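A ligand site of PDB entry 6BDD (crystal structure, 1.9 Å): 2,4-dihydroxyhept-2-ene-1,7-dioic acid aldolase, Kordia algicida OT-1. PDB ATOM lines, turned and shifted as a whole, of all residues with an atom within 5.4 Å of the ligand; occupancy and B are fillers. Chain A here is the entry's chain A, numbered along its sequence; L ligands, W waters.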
ATOM      1  N   MET A   1      10.299  28.202  26.414  1.00  0.00           N
ATOM      2  CA  MET A   1      10.366  27.871  24.998  1.00  0.00           C
ATOM      3  C   MET A   1      10.828  26.434  24.797  1.00  0.00           C
ATOM      4  O   MET A   1      11.779  25.989  25.430  1.00  0.00           O
ATOM      5  CB  MET A   1      11.315  28.840  24.271  1.00  0.00           C
ATOM      6  CG  MET A   1      11.496  28.549  22.802  1.00  0.00           C
ATOM      7  SD  MET A   1      12.066  29.995  21.887  1.00  0.00           S
ATOM      8  CE  MET A   1      10.550  30.925  21.742  1.00  0.00           C
ATOM      9  N   LYS A   2      10.137  25.712  23.916  1.00  0.00           N
ATOM     10  CA  LYS A   2      10.466  24.316  23.681  1.00  0.00           C
ATOM     11  C   LYS A   2      11.774  24.192  22.914  1.00  0.00           C
ATOM     12  O   LYS A   2      12.167  25.069  22.141  1.00  0.00           O
ATOM     13  CB  LYS A   2       9.335  23.632  22.902  1.00  0.00           C
ATOM     14  CG  LYS A   2       8.044  23.489  23.688  1.00  0.00           C
ATOM     15  CD  LYS A   2       8.279  22.843  25.046  1.00  0.00           C
ATOM     16  CE  LYS A   2       8.778  21.411  24.904  1.00  0.00           C
ATOM     17  NZ  LYS A   2       9.215  20.841  26.210  1.00  0.00           N
ATOM     18  N   ILE A   4      12.577  22.286  20.453  1.00  0.00           N
ATOM     19  CA  ILE A   4      12.470  22.179  18.996  1.00  0.00           C
ATOM     20  C   ILE A   4      12.647  23.539  18.349  1.00  0.00           C
ATOM     21  O   ILE A   4      13.186  23.641  17.234  1.00  0.00           O
ATOM     22  CB  ILE A   4      11.127  21.522  18.608  1.00  0.00           C
ATOM     23  CG1 ILE A   4      11.002  21.428  17.084  1.00  0.00           C
ATOM     24  CG2 ILE A   4       9.964  22.293  19.208  1.00  0.00           C
ATOM     25  CD1 ILE A   4      12.006  20.484  16.455  1.00  0.00           C
ATOM     26  N   ILE A   5      12.217  24.606  19.019  1.00  0.00           N
ATOM     27  CA  ILE A   5      12.415  25.947  18.488  1.00  0.00           C
ATOM     28  C   ILE A   5      13.904  26.282  18.436  1.00  0.00           C
ATOM     29  O   ILE A   5      14.369  26.954  17.505  1.00  0.00           O
ATOM     30  CB  ILE A   5      11.625  26.979  19.313  1.00  0.00           C
ATOM     31  CG1 ILE A   5      10.174  26.533  19.480  1.00  0.00           C
ATOM     32  CG2 ILE A   5      11.701  28.351  18.668  1.00  0.00           C
ATOM     33  CD1 ILE A   5       9.407  26.492  18.178  1.00  0.00           C
ATOM     34  N   PHE A  74      10.155  27.050   9.564  1.00  0.00           N
ATOM     35  CA  PHE A  74       9.576  26.222  10.605  1.00  0.00           C
ATOM     36  C   PHE A  74       8.180  25.719  10.245  1.00  0.00           C
ATOM     37  O   PHE A  74       7.751  24.702  10.785  1.00  0.00           O
ATOM     38  CB  PHE A  74       9.515  27.000  11.928  1.00  0.00           C
ATOM     39  CG  PHE A  74       9.180  26.133  13.118  1.00  0.00           C
ATOM     40  CD1 PHE A  74      10.165  25.378  13.735  1.00  0.00           C
ATOM     41  CD2 PHE A  74       7.891  26.082  13.605  1.00  0.00           C
ATOM     42  CE1 PHE A  74       9.865  24.581  14.820  1.00  0.00           C
ATOM     43  CE2 PHE A  74       7.579  25.290  14.696  1.00  0.00           C
ATOM     44  CZ  PHE A  74       8.569  24.536  15.304  1.00  0.00           C
ATOM     45  N   PHE A  75       7.471  26.413   9.351  1.00  0.00           N
ATOM     46  CA  PHE A  75       6.163  25.919   8.927  1.00  0.00           C
ATOM     47  C   PHE A  75       6.277  24.584   8.196  1.00  0.00           C
ATOM     48  O   PHE A  75       5.374  23.753   8.293  1.00  0.00           O
ATOM     49  CB  PHE A  75       5.473  26.947   8.040  1.00  0.00           C
ATOM     50  CG  PHE A  75       4.021  26.634   7.762  1.00  0.00           C
ATOM     51  CD1 PHE A  75       3.031  27.058   8.623  1.00  0.00           C
ATOM     52  CD2 PHE A  75       3.664  25.898   6.639  1.00  0.00           C
ATOM     53  CE1 PHE A  75       1.704  26.775   8.379  1.00  0.00           C
ATOM     54  CE2 PHE A  75       2.337  25.610   6.382  1.00  0.00           C
ATOM     55  CZ  PHE A  75       1.357  26.048   7.252  1.00  0.00           C
ATOM     56  N   ILE A  78       6.313  22.104  10.743  1.00  0.00           N
ATOM     57  CA  ILE A  78       4.940  21.879  11.186  1.00  0.00           C
ATOM     58  C   ILE A  78       4.181  21.026  10.176  1.00  0.00           C
ATOM     59  O   ILE A  78       3.410  20.134  10.551  1.00  0.00           O
ATOM     60  CB  ILE A  78       4.250  23.228  11.445  1.00  0.00           C
ATOM     61  CG1 ILE A  78       4.787  23.886  12.717  1.00  0.00           C
ATOM     62  CG2 ILE A  78       2.742  23.052  11.522  1.00  0.00           C
ATOM     63  CD1 ILE A  78       4.232  25.272  12.970  1.00  0.00           C
ATOM     64  N   TYR A  82       2.865  17.480  11.876  1.00  0.00           N
ATOM     65  CA  TYR A  82       1.440  17.379  12.199  1.00  0.00           C
ATOM     66  C   TYR A  82       0.607  17.639  10.939  1.00  0.00           C
ATOM     67  O   TYR A  82      -0.088  18.660  10.844  1.00  0.00           O
ATOM     68  CB  TYR A  82       1.068  18.359  13.311  1.00  0.00           C
ATOM     69  CG  TYR A  82       1.898  18.186  14.565  1.00  0.00           C
ATOM     70  CD1 TYR A  82       1.571  17.223  15.511  1.00  0.00           C
ATOM     71  CD2 TYR A  82       3.022  18.966  14.791  1.00  0.00           C
ATOM     72  CE1 TYR A  82       2.328  17.060  16.653  1.00  0.00           C
ATOM     73  CE2 TYR A  82       3.789  18.812  15.928  1.00  0.00           C
ATOM     74  CZ  TYR A  82       3.431  17.854  16.858  1.00  0.00           C
ATOM     75  OH  TYR A  82       4.200  17.686  17.993  1.00  0.00           O
ATOM     76  N   LEU A  85      -3.350  17.686  11.621  1.00  0.00           N
ATOM     77  CA  LEU A  85      -3.896  18.935  12.145  1.00  0.00           C
ATOM     78  C   LEU A  85      -4.120  19.941  11.020  1.00  0.00           C
ATOM     79  O   LEU A  85      -5.142  20.632  10.996  1.00  0.00           O
ATOM     80  CB  LEU A  85      -2.953  19.515  13.202  1.00  0.00           C
ATOM     81  CG  LEU A  85      -3.428  20.762  13.934  1.00  0.00           C
ATOM     82  CD1 LEU A  85      -4.836  20.569  14.471  1.00  0.00           C
ATOM     83  CD2 LEU A  85      -2.471  21.110  15.065  1.00  0.00           C
ATOM     84  N   LEU A  86      -3.164  20.036  10.081  1.00  0.00           N
ATOM     85  CA  LEU A  86      -3.337  20.943   8.953  1.00  0.00           C
ATOM     86  C   LEU A  86      -4.433  20.475   8.008  1.00  0.00           C
ATOM     87  O   LEU A  86      -5.106  21.290   7.378  1.00  0.00           O
ATOM     88  CB  LEU A  86      -2.022  21.093   8.195  1.00  0.00           C
ATOM     89  CG  LEU A  86      -1.142  22.284   8.561  1.00  0.00           C
ATOM     90  CD1 LEU A  86      -0.424  22.033   9.884  1.00  0.00           C
ATOM     91  CD2 LEU A  86      -0.143  22.589   7.459  1.00  0.00           C
ATOM     92  N   MET A  95      -8.219  28.778   9.139  1.00  0.00           N
ATOM     93  CA  MET A  95      -7.179  28.196   9.983  1.00  0.00           C
ATOM     94  C   MET A  95      -6.571  29.246  10.902  1.00  0.00           C
ATOM     95  O   MET A  95      -6.365  28.993  12.097  1.00  0.00           O
ATOM     96  CB  MET A  95      -6.105  27.549   9.109  1.00  0.00           C
ATOM     97  CG  MET A  95      -4.900  27.045   9.892  1.00  0.00           C
ATOM     98  SD  MET A  95      -3.741  26.121   8.873  1.00  0.00           S
ATOM     99  CE  MET A  95      -2.391  25.887  10.021  1.00  0.00           C
ATOM    100  N   LEU A  96      -6.265  30.438  10.365  1.00  0.00           N
ATOM    101  CA  LEU A  96      -5.686  31.490  11.184  1.00  0.00           C
ATOM    102  C   LEU A  96      -6.662  31.973  12.257  1.00  0.00           C
ATOM    103  O   LEU A  96      -6.236  32.326  13.357  1.00  0.00           O
ATOM    104  CB  LEU A  96      -5.251  32.664  10.304  1.00  0.00           C
ATOM    105  CG  LEU A  96      -4.075  32.391   9.352  1.00  0.00           C
ATOM    106  CD1 LEU A  96      -3.713  33.659   8.593  1.00  0.00           C
ATOM    107  CD2 LEU A  96      -2.878  31.858  10.124  1.00  0.00           C
ATOM    108  N   ILE A  99      -6.399  29.564  15.504  1.00  0.00           N
ATOM    109  CA  ILE A  99      -5.147  29.315  16.220  1.00  0.00           C
ATOM    110  C   ILE A  99      -5.393  29.267  17.715  1.00  0.00           C
ATOM    111  O   ILE A  99      -4.869  28.395  18.420  1.00  0.00           O
ATOM    112  CB  ILE A  99      -4.107  30.386  15.857  1.00  0.00           C
ATOM    113  CG1 ILE A  99      -3.762  30.328  14.362  1.00  0.00           C
ATOM    114  CG2 ILE A  99      -2.845  30.216  16.694  1.00  0.00           C
ATOM    115  CD1 ILE A  99      -3.152  31.603  13.848  1.00  0.00           C
ATOM    116  N   ILE A 103      -5.899  25.268  17.393  1.00  0.00           N
ATOM    117  CA  ILE A 103      -4.545  24.872  17.031  1.00  0.00           C
ATOM    118  C   ILE A 103      -3.629  24.869  18.245  1.00  0.00           C
ATOM    119  O   ILE A 103      -3.105  23.827  18.661  1.00  0.00           O
ATOM    120  CB  ILE A 103      -3.987  25.765  15.909  1.00  0.00           C
ATOM    121  CG1 ILE A 103      -4.769  25.541  14.614  1.00  0.00           C
ATOM    122  CG2 ILE A 103      -2.512  25.506  15.698  1.00  0.00           C
ATOM    123  CD1 ILE A 103      -4.249  26.361  13.453  1.00  0.00           C
ATOM    124  N   HIS A 104      -3.430  26.047  18.854  1.00  0.00           N
ATOM    125  CA  HIS A 104      -2.566  26.122  20.020  1.00  0.00           C
ATOM    126  C   HIS A 104      -3.196  25.490  21.254  1.00  0.00           C
ATOM    127  O   HIS A 104      -2.500  25.293  22.256  1.00  0.00           O
ATOM    128  CB  HIS A 104      -2.176  27.580  20.285  1.00  0.00           C
ATOM    129  CG  HIS A 104      -1.041  28.067  19.438  1.00  0.00           C
ATOM    130  ND1 HIS A 104      -0.750  29.408  19.284  1.00  0.00           N
ATOM    131  CD2 HIS A 104      -0.123  27.390  18.713  1.00  0.00           C
ATOM    132  CE1 HIS A 104       0.303  29.534  18.494  1.00  0.00           C
ATOM    133  NE2 HIS A 104       0.698  28.326  18.128  1.00  0.00           N
ATOM    134  N   VAL A 107      -1.665  22.183  20.770  1.00  0.00           N
ATOM    135  CA  VAL A 107      -0.238  22.289  21.104  1.00  0.00           C
ATOM    136  C   VAL A 107      -0.040  22.195  22.615  1.00  0.00           C
ATOM    137  O   VAL A 107       0.924  21.586  23.087  1.00  0.00           O
ATOM    138  CB  VAL A 107       0.344  23.603  20.535  1.00  0.00           C
ATOM    139  CG1 VAL A 107       1.817  23.716  20.874  1.00  0.00           C
ATOM    140  CG2 VAL A 107       0.124  23.663  19.037  1.00  0.00           C
ATOM    141  N   TYR A 111       2.356  19.773  24.569  1.00  0.00           N
ATOM    142  CA  TYR A 111       3.351  20.399  25.455  1.00  0.00           C
ATOM    143  C   TYR A 111       2.615  21.246  26.472  1.00  0.00           C
ATOM    144  O   TYR A 111       2.296  22.414  26.221  1.00  0.00           O
ATOM    145  CB  TYR A 111       4.341  21.239  24.652  1.00  0.00           C
ATOM    146  CG  TYR A 111       4.986  20.497  23.498  1.00  0.00           C
ATOM    147  CD1 TYR A 111       5.996  19.568  23.720  1.00  0.00           C
ATOM    148  CD2 TYR A 111       4.588  20.734  22.185  1.00  0.00           C
ATOM    149  CE1 TYR A 111       6.595  18.897  22.674  1.00  0.00           C
ATOM    150  CE2 TYR A 111       5.175  20.062  21.131  1.00  0.00           C
ATOM    151  CZ  TYR A 111       6.184  19.144  21.379  1.00  0.00           C
ATOM    152  OH  TYR A 111       6.766  18.470  20.334  1.00  0.00           O
ATOM    153  N   ASP A 113       3.752  22.653  29.065  1.00  0.00           N
ATOM    154  CA  ASP A 113       4.606  23.746  29.487  1.00  0.00           C
ATOM    155  C   ASP A 113       4.980  24.677  28.347  1.00  0.00           C
ATOM    156  O   ASP A 113       5.960  25.430  28.445  1.00  0.00           O
ATOM    157  CB  ASP A 113       5.870  23.195  30.153  1.00  0.00           C
ATOM    158  CG  ASP A 113       6.698  22.352  29.203  1.00  0.00           C
ATOM    159  OD1 ASP A 113       6.122  21.789  28.251  1.00  0.00           O
ATOM    160  OD2 ASP A 113       7.926  22.239  29.426  1.00  0.00           O
ATOM    161  N   ALA A 114       4.229  24.648  27.248  1.00  0.00           N
ATOM    162  CA  ALA A 114       4.536  25.489  26.106  1.00  0.00           C
ATOM    163  C   ALA A 114       4.235  26.946  26.409  1.00  0.00           C
ATOM    164  O   ALA A 114       3.278  27.264  27.122  1.00  0.00           O
ATOM    165  CB  ALA A 114       3.739  25.029  24.878  1.00  0.00           C
ATOM    166  N   GLU A 115       5.068  27.834  25.867  1.00  0.00           N
ATOM    167  CA  GLU A 115       4.870  29.281  25.991  1.00  0.00           C
ATOM    168  C   GLU A 115       4.282  29.771  24.670  1.00  0.00           C
ATOM    169  O   GLU A 115       4.985  29.919  23.676  1.00  0.00           O
ATOM    170  CB  GLU A 115       6.190  29.979  26.315  1.00  0.00           C
ATOM    171  CG  GLU A 115       6.851  29.492  27.597  1.00  0.00           C
ATOM    172  CD  GLU A 115       8.155  30.200  27.879  1.00  0.00           C
ATOM    173  OE1 GLU A 115       8.911  30.467  26.919  1.00  0.00           O
ATOM    174  OE2 GLU A 115       8.419  30.501  29.059  1.00  0.00           O
ATOM    175  N   LEU A 116       2.978  30.027  24.685  1.00  0.00           N
ATOM    176  CA  LEU A 116       2.262  30.373  23.468  1.00  0.00           C
ATOM    177  C   LEU A 116       1.703  31.790  23.547  1.00  0.00           C
ATOM    178  O   LEU A 116       1.418  32.288  24.646  1.00  0.00           O
ATOM    179  CB  LEU A 116       1.101  29.388  23.220  1.00  0.00           C
ATOM    180  CG  LEU A 116       1.508  27.926  23.028  1.00  0.00           C
ATOM    181  CD1 LEU A 116       0.287  27.020  23.082  1.00  0.00           C
ATOM    182  CD2 LEU A 116       2.259  27.757  21.714  1.00  0.00           C
ATOM    183  N   PRO A 117       1.546  32.467  22.422  1.00  0.00           N
ATOM    184  CA  PRO A 117       0.922  33.791  22.416  1.00  0.00           C
ATOM    185  C   PRO A 117      -0.597  33.657  22.437  1.00  0.00           C
ATOM    186  O   PRO A 117      -1.150  32.558  22.420  1.00  0.00           O
ATOM    187  CB  PRO A 117       1.417  34.397  21.107  1.00  0.00           C
ATOM    188  CG  PRO A 117       1.542  33.217  20.204  1.00  0.00           C
ATOM    189  CD  PRO A 117       1.956  32.046  21.071  1.00  0.00           C
ATOM    190  N   PHE A 119      -4.152  35.086  20.460  1.00  0.00           N
ATOM    191  CA  PHE A 119      -4.733  35.723  19.285  1.00  0.00           C
ATOM    192  C   PHE A 119      -6.209  35.969  19.540  1.00  0.00           C
ATOM    193  O   PHE A 119      -6.932  35.051  19.950  1.00  0.00           O
ATOM    194  CB  PHE A 119      -4.551  34.845  18.036  1.00  0.00           C
ATOM    195  CG  PHE A 119      -3.167  34.921  17.433  1.00  0.00           C
ATOM    196  CD1 PHE A 119      -2.798  35.999  16.645  1.00  0.00           C
ATOM    197  CD2 PHE A 119      -2.261  33.904  17.644  1.00  0.00           C
ATOM    198  CE1 PHE A 119      -1.539  36.062  16.083  1.00  0.00           C
ATOM    199  CE2 PHE A 119      -0.995  33.967  17.098  1.00  0.00           C
ATOM    200  CZ  PHE A 119      -0.636  35.035  16.314  1.00  0.00           C
ATOM    201  N   TYR A 133      -2.525  40.215  18.329  1.00  0.00           N
ATOM    202  CA  TYR A 133      -1.479  39.334  18.822  1.00  0.00           C
ATOM    203  C   TYR A 133      -0.929  39.896  20.127  1.00  0.00           C
ATOM    204  O   TYR A 133      -0.652  41.092  20.216  1.00  0.00           O
ATOM    205  CB  TYR A 133      -0.360  39.195  17.784  1.00  0.00           C
ATOM    206  CG  TYR A 133       0.939  38.633  18.301  1.00  0.00           C
ATOM    207  CD1 TYR A 133       1.172  37.268  18.312  1.00  0.00           C
ATOM    208  CD2 TYR A 133       1.950  39.465  18.757  1.00  0.00           C
ATOM    209  CE1 TYR A 133       2.360  36.747  18.772  1.00  0.00           C
ATOM    210  CE2 TYR A 133       3.144  38.957  19.235  1.00  0.00           C
ATOM    211  CZ  TYR A 133       3.340  37.594  19.237  1.00  0.00           C
ATOM    212  OH  TYR A 133       4.534  37.081  19.702  1.00  0.00           O
ATOM    213  N   SER A 135       1.937  38.841  23.265  1.00  0.00           N
ATOM    214  CA  SER A 135       2.968  37.965  23.810  1.00  0.00           C
ATOM    215  C   SER A 135       4.116  38.791  24.370  1.00  0.00           C
ATOM    216  O   SER A 135       4.613  39.706  23.705  1.00  0.00           O
ATOM    217  CB  SER A 135       3.482  36.994  22.750  1.00  0.00           C
ATOM    218  OG  SER A 135       4.695  36.388  23.169  1.00  0.00           O
ATOM    219  N   ARG A 137       7.014  37.970  24.501  1.00  0.00           N
ATOM    220  CA  ARG A 137       8.198  37.670  23.715  1.00  0.00           C
ATOM    221  C   ARG A 137       8.294  38.496  22.431  1.00  0.00           C
ATOM    222  O   ARG A 137       9.342  38.494  21.787  1.00  0.00           O
ATOM    223  CB  ARG A 137       8.239  36.175  23.378  1.00  0.00           C
ATOM    224  CG  ARG A 137       8.386  35.281  24.601  1.00  0.00           C
ATOM    225  CD  ARG A 137       8.056  33.838  24.292  1.00  0.00           C
ATOM    226  NE  ARG A 137       6.616  33.612  24.184  1.00  0.00           N
ATOM    227  CZ  ARG A 137       5.800  33.418  25.219  1.00  0.00           C
ATOM    228  NH1 ARG A 137       6.286  33.430  26.453  1.00  0.00           N
ATOM    229  NH2 ARG A 137       4.507  33.222  25.017  1.00  0.00           N
ATOM    230  N   MET A 139       7.212  38.205  19.407  1.00  0.00           N
ATOM    231  CA  MET A 139       7.586  37.430  18.225  1.00  0.00           C
ATOM    232  C   MET A 139       6.529  37.545  17.130  1.00  0.00           C
ATOM    233  O   MET A 139       6.110  36.561  16.530  1.00  0.00           O
ATOM    234  CB  MET A 139       7.815  35.970  18.604  1.00  0.00           C
ATOM    235  CG  MET A 139       8.957  35.761  19.586  1.00  0.00           C
ATOM    236  SD  MET A 139       9.168  34.030  20.069  1.00  0.00           S
ATOM    237  CE  MET A 139       9.475  33.270  18.482  1.00  0.00           C
ATOM    238  N   PHE A 142       7.605  36.130  13.842  1.00  0.00           N
ATOM    239  CA  PHE A 142       7.493  34.671  13.803  1.00  0.00           C
ATOM    240  C   PHE A 142       6.074  34.261  13.427  1.00  0.00           C
ATOM    241  O   PHE A 142       5.888  33.327  12.633  1.00  0.00           O
ATOM    242  CB  PHE A 142       7.894  34.082  15.155  1.00  0.00           C
ATOM    243  CG  PHE A 142       7.962  32.581  15.166  1.00  0.00           C
ATOM    244  CD1 PHE A 142       9.089  31.927  14.678  1.00  0.00           C
ATOM    245  CD2 PHE A 142       6.917  31.824  15.658  1.00  0.00           C
ATOM    246  CE1 PHE A 142       9.160  30.549  14.684  1.00  0.00           C
ATOM    247  CE2 PHE A 142       6.982  30.445  15.673  1.00  0.00           C
ATOM    248  CZ  PHE A 142       8.102  29.797  15.182  1.00  0.00           C
ATOM    249  N   GLY A 143       5.068  34.944  13.958  1.00  0.00           N
ATOM    250  CA  GLY A 143       3.704  34.685  13.543  1.00  0.00           C
ATOM    251  C   GLY A 143       3.432  35.104  12.110  1.00  0.00           C
ATOM    252  O   GLY A 143       2.644  34.464  11.416  1.00  0.00           O
ATOM    253  N   LEU A 146       4.658  32.334   9.760  1.00  0.00           N
ATOM    254  CA  LEU A 146       3.721  31.210   9.733  1.00  0.00           C
ATOM    255  C   LEU A 146       2.438  31.567   8.987  1.00  0.00           C
ATOM    256  O   LEU A 146       1.842  30.706   8.334  1.00  0.00           O
ATOM    257  CB  LEU A 146       3.400  30.754  11.158  1.00  0.00           C
ATOM    258  CG  LEU A 146       4.592  30.276  12.000  1.00  0.00           C
ATOM    259  CD1 LEU A 146       4.145  29.904  13.404  1.00  0.00           C
ATOM    260  CD2 LEU A 146       5.292  29.107  11.338  1.00  0.00           C
ATOM    261  N   MET A 147       2.000  32.828   9.078  1.00  0.00           N
ATOM    262  CA  MET A 147       0.848  33.268   8.300  1.00  0.00           C
ATOM    263  C   MET A 147       1.140  33.214   6.809  1.00  0.00           C
ATOM    264  O   MET A 147       0.294  32.780   6.022  1.00  0.00           O
ATOM    265  CB  MET A 147       0.448  34.688   8.701  1.00  0.00           C
ATOM    266  CG  MET A 147      -0.354  34.772   9.988  1.00  0.00           C
ATOM    267  SD  MET A 147      -0.625  36.457  10.564  1.00  0.00           S
ATOM    268  CE  MET A 147      -1.081  36.172  12.269  1.00  0.00           C
ATOM    269  N   THR A 150       1.070  29.705   5.746  1.00  0.00           N
ATOM    270  CA  THR A 150      -0.284  29.178   5.833  1.00  0.00           C
ATOM    271  C   THR A 150      -1.051  29.453   4.546  1.00  0.00           C
ATOM    272  O   THR A 150      -1.702  28.571   3.985  1.00  0.00           O
ATOM    273  CB  THR A 150      -1.015  29.784   7.035  1.00  0.00           C
ATOM    274  OG1 THR A 150      -0.413  29.312   8.249  1.00  0.00           O
ATOM    275  CG2 THR A 150      -2.481  29.397   7.016  1.00  0.00           C
HETATM  276  C1  LIG L   1       4.776  29.182  19.132  1.00  0.00           C
HETATM  277  C2  LIG L   1       2.964  24.997  17.509  1.00  0.00           C
HETATM  278  C3  LIG L   1       0.426  27.357  14.147  1.00  0.00           C
HETATM  279  C4  LIG L   1       1.791  31.510  16.161  1.00  0.00           C
HETATM  280  C5  LIG L   1       4.569  27.840  18.921  1.00  0.00           C
HETATM  281  C6  LIG L   1       5.327  26.761  19.516  1.00  0.00           C
HETATM  282  C7  LIG L   1       4.827  25.614  19.067  1.00  0.00           C
HETATM  283  C8  LIG L   1       3.731  25.927  18.173  1.00  0.00           C
HETATM  284  C9  LIG L   1       5.334  24.208  19.435  1.00  0.00           C
HETATM  285  C10 LIG L   1       6.507  26.920  20.499  1.00  0.00           C
HETATM  286  C11 LIG L   1       5.974  26.987  21.919  1.00  0.00           C
HETATM  287  C12 LIG L   1       7.127  26.990  22.897  1.00  0.00           C
HETATM  288  O1  LIG L   1       6.868  26.968  24.128  1.00  0.00           O
HETATM  289  O2  LIG L   1       8.300  27.004  22.439  1.00  0.00           O
HETATM  290  C13 LIG L   1       2.167  25.282  16.431  1.00  0.00           C
HETATM  291  C14 LIG L   1       1.574  24.295  15.547  1.00  0.00           C
HETATM  292  C15 LIG L   1       0.874  24.952  14.615  1.00  0.00           C
HETATM  293  C16 LIG L   1       1.008  26.366  14.895  1.00  0.00           C
HETATM  294  C17 LIG L   1       1.767  22.770  15.723  1.00  0.00           C
HETATM  295  C18 LIG L   1       0.034  24.414  13.427  1.00  0.00           C
HETATM  296  C19 LIG L   1      -0.264  23.129  13.221  1.00  0.00           C
HETATM  297  C20 LIG L   1       0.642  28.684  14.372  1.00  0.00           C
HETATM  298  C21 LIG L   1       0.232  29.758  13.485  1.00  0.00           C
HETATM  299  C22 LIG L   1       0.621  30.908  14.046  1.00  0.00           C
HETATM  300  C23 LIG L   1       1.264  30.588  15.297  1.00  0.00           C
HETATM  301  C24 LIG L   1      -0.498  29.520  12.135  1.00  0.00           C
HETATM  302  C25 LIG L   1       0.449  32.376  13.573  1.00  0.00           C
HETATM  303  C26 LIG L   1      -0.253  32.725  12.508  1.00  0.00           C
HETATM  304  C27 LIG L   1       2.808  31.239  17.029  1.00  0.00           C
HETATM  305  C28 LIG L   1       3.770  32.196  17.509  1.00  0.00           C
HETATM  306  C29 LIG L   1       4.601  31.561  18.334  1.00  0.00           C
HETATM  307  C30 LIG L   1       4.184  30.169  18.402  1.00  0.00           C
HETATM  308  C31 LIG L   1       3.823  33.694  17.141  1.00  0.00           C
HETATM  309  C32 LIG L   1       5.781  32.222  19.078  1.00  0.00           C
HETATM  310  C33 LIG L   1       5.518  32.279  20.574  1.00  0.00           C
HETATM  311  C34 LIG L   1       5.060  33.661  20.967  1.00  0.00           C
HETATM  312  O3  LIG L   1       4.845  34.509  20.061  1.00  0.00           O
HETATM  313  O4  LIG L   1       4.910  33.926  22.188  1.00  0.00           O
HETATM  314  N1  LIG L   1       3.592  27.303  18.090  1.00  0.00           N
HETATM  315  N2  LIG L   1       1.815  26.555  16.005  1.00  0.00           N
HETATM  316  N3  LIG L   1       1.272  29.220  15.482  1.00  0.00           N
HETATM  317  N4  LIG L   1       3.081  29.993  17.580  1.00  0.00           N
HETATM  318 FE1  LIG L   1       2.293  28.265  16.917  1.00  0.00          FE
HETATM  319  O   HOH W   1       7.987  26.357  26.654  1.00  0.00           O
HETATM  320  O   HOH W   2       7.699  30.185  23.415  1.00  0.00           O
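The backbone NH (N) of Lys 2 sits at hydrogen-bond distance from an oxygen (O2) of the ligand.
The side-chain hydroxyl (OH) of Tyr 133 sits at hydrogen-bond distance from an oxygen (O3) of the ligand.
The guanidinium group (NE) of Arg 137 lies within salt-bridge range of an oxygen (O4) of the ligand, at 2.6 Å.
An iron atom (FE1) of the ligand is bound by a ring nitrogen (NE2) of His 104 (2.0 Å).
The backbone NH of Glu 115 sits at hydrogen-bond distance from an oxygen (O1) of the ligand, 2.6 Å away.
OG of Ser 135 lies within hydrogen-bond range of O4 of the ligand.
The backbone carbonyl oxygen (O) of Ile 99 is in hydrogen-bond range of the backbone NH (N) of His 104 (2.8 Å).
The side-chain hydroxyl of Thr 150 is in hydrogen-bond range of the backbone carbonyl oxygen of Leu 146.
OE1 of Glu 115 lies within hydrogen-bond range of N of Met 1.
NH2 of Arg 137 is in hydrogen-bond range of O of Leu 116.
NZ of Lys 2 lies within salt-bridge range of OD2 of Asp 113 (3.7 Å).
The side-chain hydroxyl (OH) of Tyr 133 lies within hydrogen-bond range of the backbone NH (N) of Met 139.
The guanidinium group (NH1) of Arg 137 is in salt-bridge range of the side-chain carboxylate (OE1) of Glu 115.
The backbone NH (N) of Arg 137 sits close to the side-chain hydroxyl (OG) of Ser 135.
Met 1 touches the ligand.
Ile 5 touches the ligand (CG1 to O2, 3.5 Å).
Ile 78 touches the ligand (CG2 to C19, 3.5 Å).
Leu 85 touches the ligand (CD2 to C19, 3.5 Å).
Leu 86 touches the ligand (CD1 to C19, 3.5 Å).
CD2 of Leu 96 touches C26 of the ligand (3.7 Å).
CD1 of Ile 99 touches C26 of the ligand, 3.4 Å away.
Ile 103 touches the ligand.
Val 107 touches the ligand.
Ala 114 touches the ligand (CA to O1, 3.4 Å).
Leu 116 touches the ligand (CD2 to C5, 3.6 Å).
Pro 117 touches the ligand (CD to C34, 3.5 Å).
Phe 119 touches the ligand (CE2 to C4, 3.8 Å).
Met 139 touches the ligand (CB to O3, 3.6 Å).
Phe 142 touches the ligand.
O of Gly 143 touches C26 of the ligand (3.6 Å).
CD1 of Leu 146 touches C23 of the ligand (3.5 Å).
Met 147 touches the ligand (CG to C26, 3.2 Å).
Thr 150 touches the ligand.
Hydrophobic or aromatic side chains that line the ligand: Met 1, Ile 5, Ile 78, Leu 85, Leu 86, Leu 96, Ile 99, Ile 103, His 104, Val 107, Ala 114, Leu 116, Pro 117, Phe 119, Tyr 133, Met 139, Phe 142, Leu 146 and Met 147.
25 residues have an atom within 4 Å of the ligand: Met 1, Lys 2, Ile 5, Ile 78, Leu 85, Leu 86, Leu 96, Ile 99, Ile 103, His 104, Val 107, Ala 114, Glu 115, Leu 116, Pro 117, Phe 119, Tyr 133, Ser 135, Arg 137, Met 139, Phe 142, Gly 143, Leu 146, Met 147 and Thr 150.
Water W1 lies within hydrogen-bond range of an oxygen (O1) of the ligand, the backbone carbonyl oxygen (O) of Asp 113, the backbone NH (N) of Met 1 and the backbone NH (N) of Glu 115.
Water W2 lies within hydrogen-bond range of the backbone carbonyl oxygen of Glu 115 (2.7 Å) and an oxygen (O2) of the ligand (3.4 Å).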
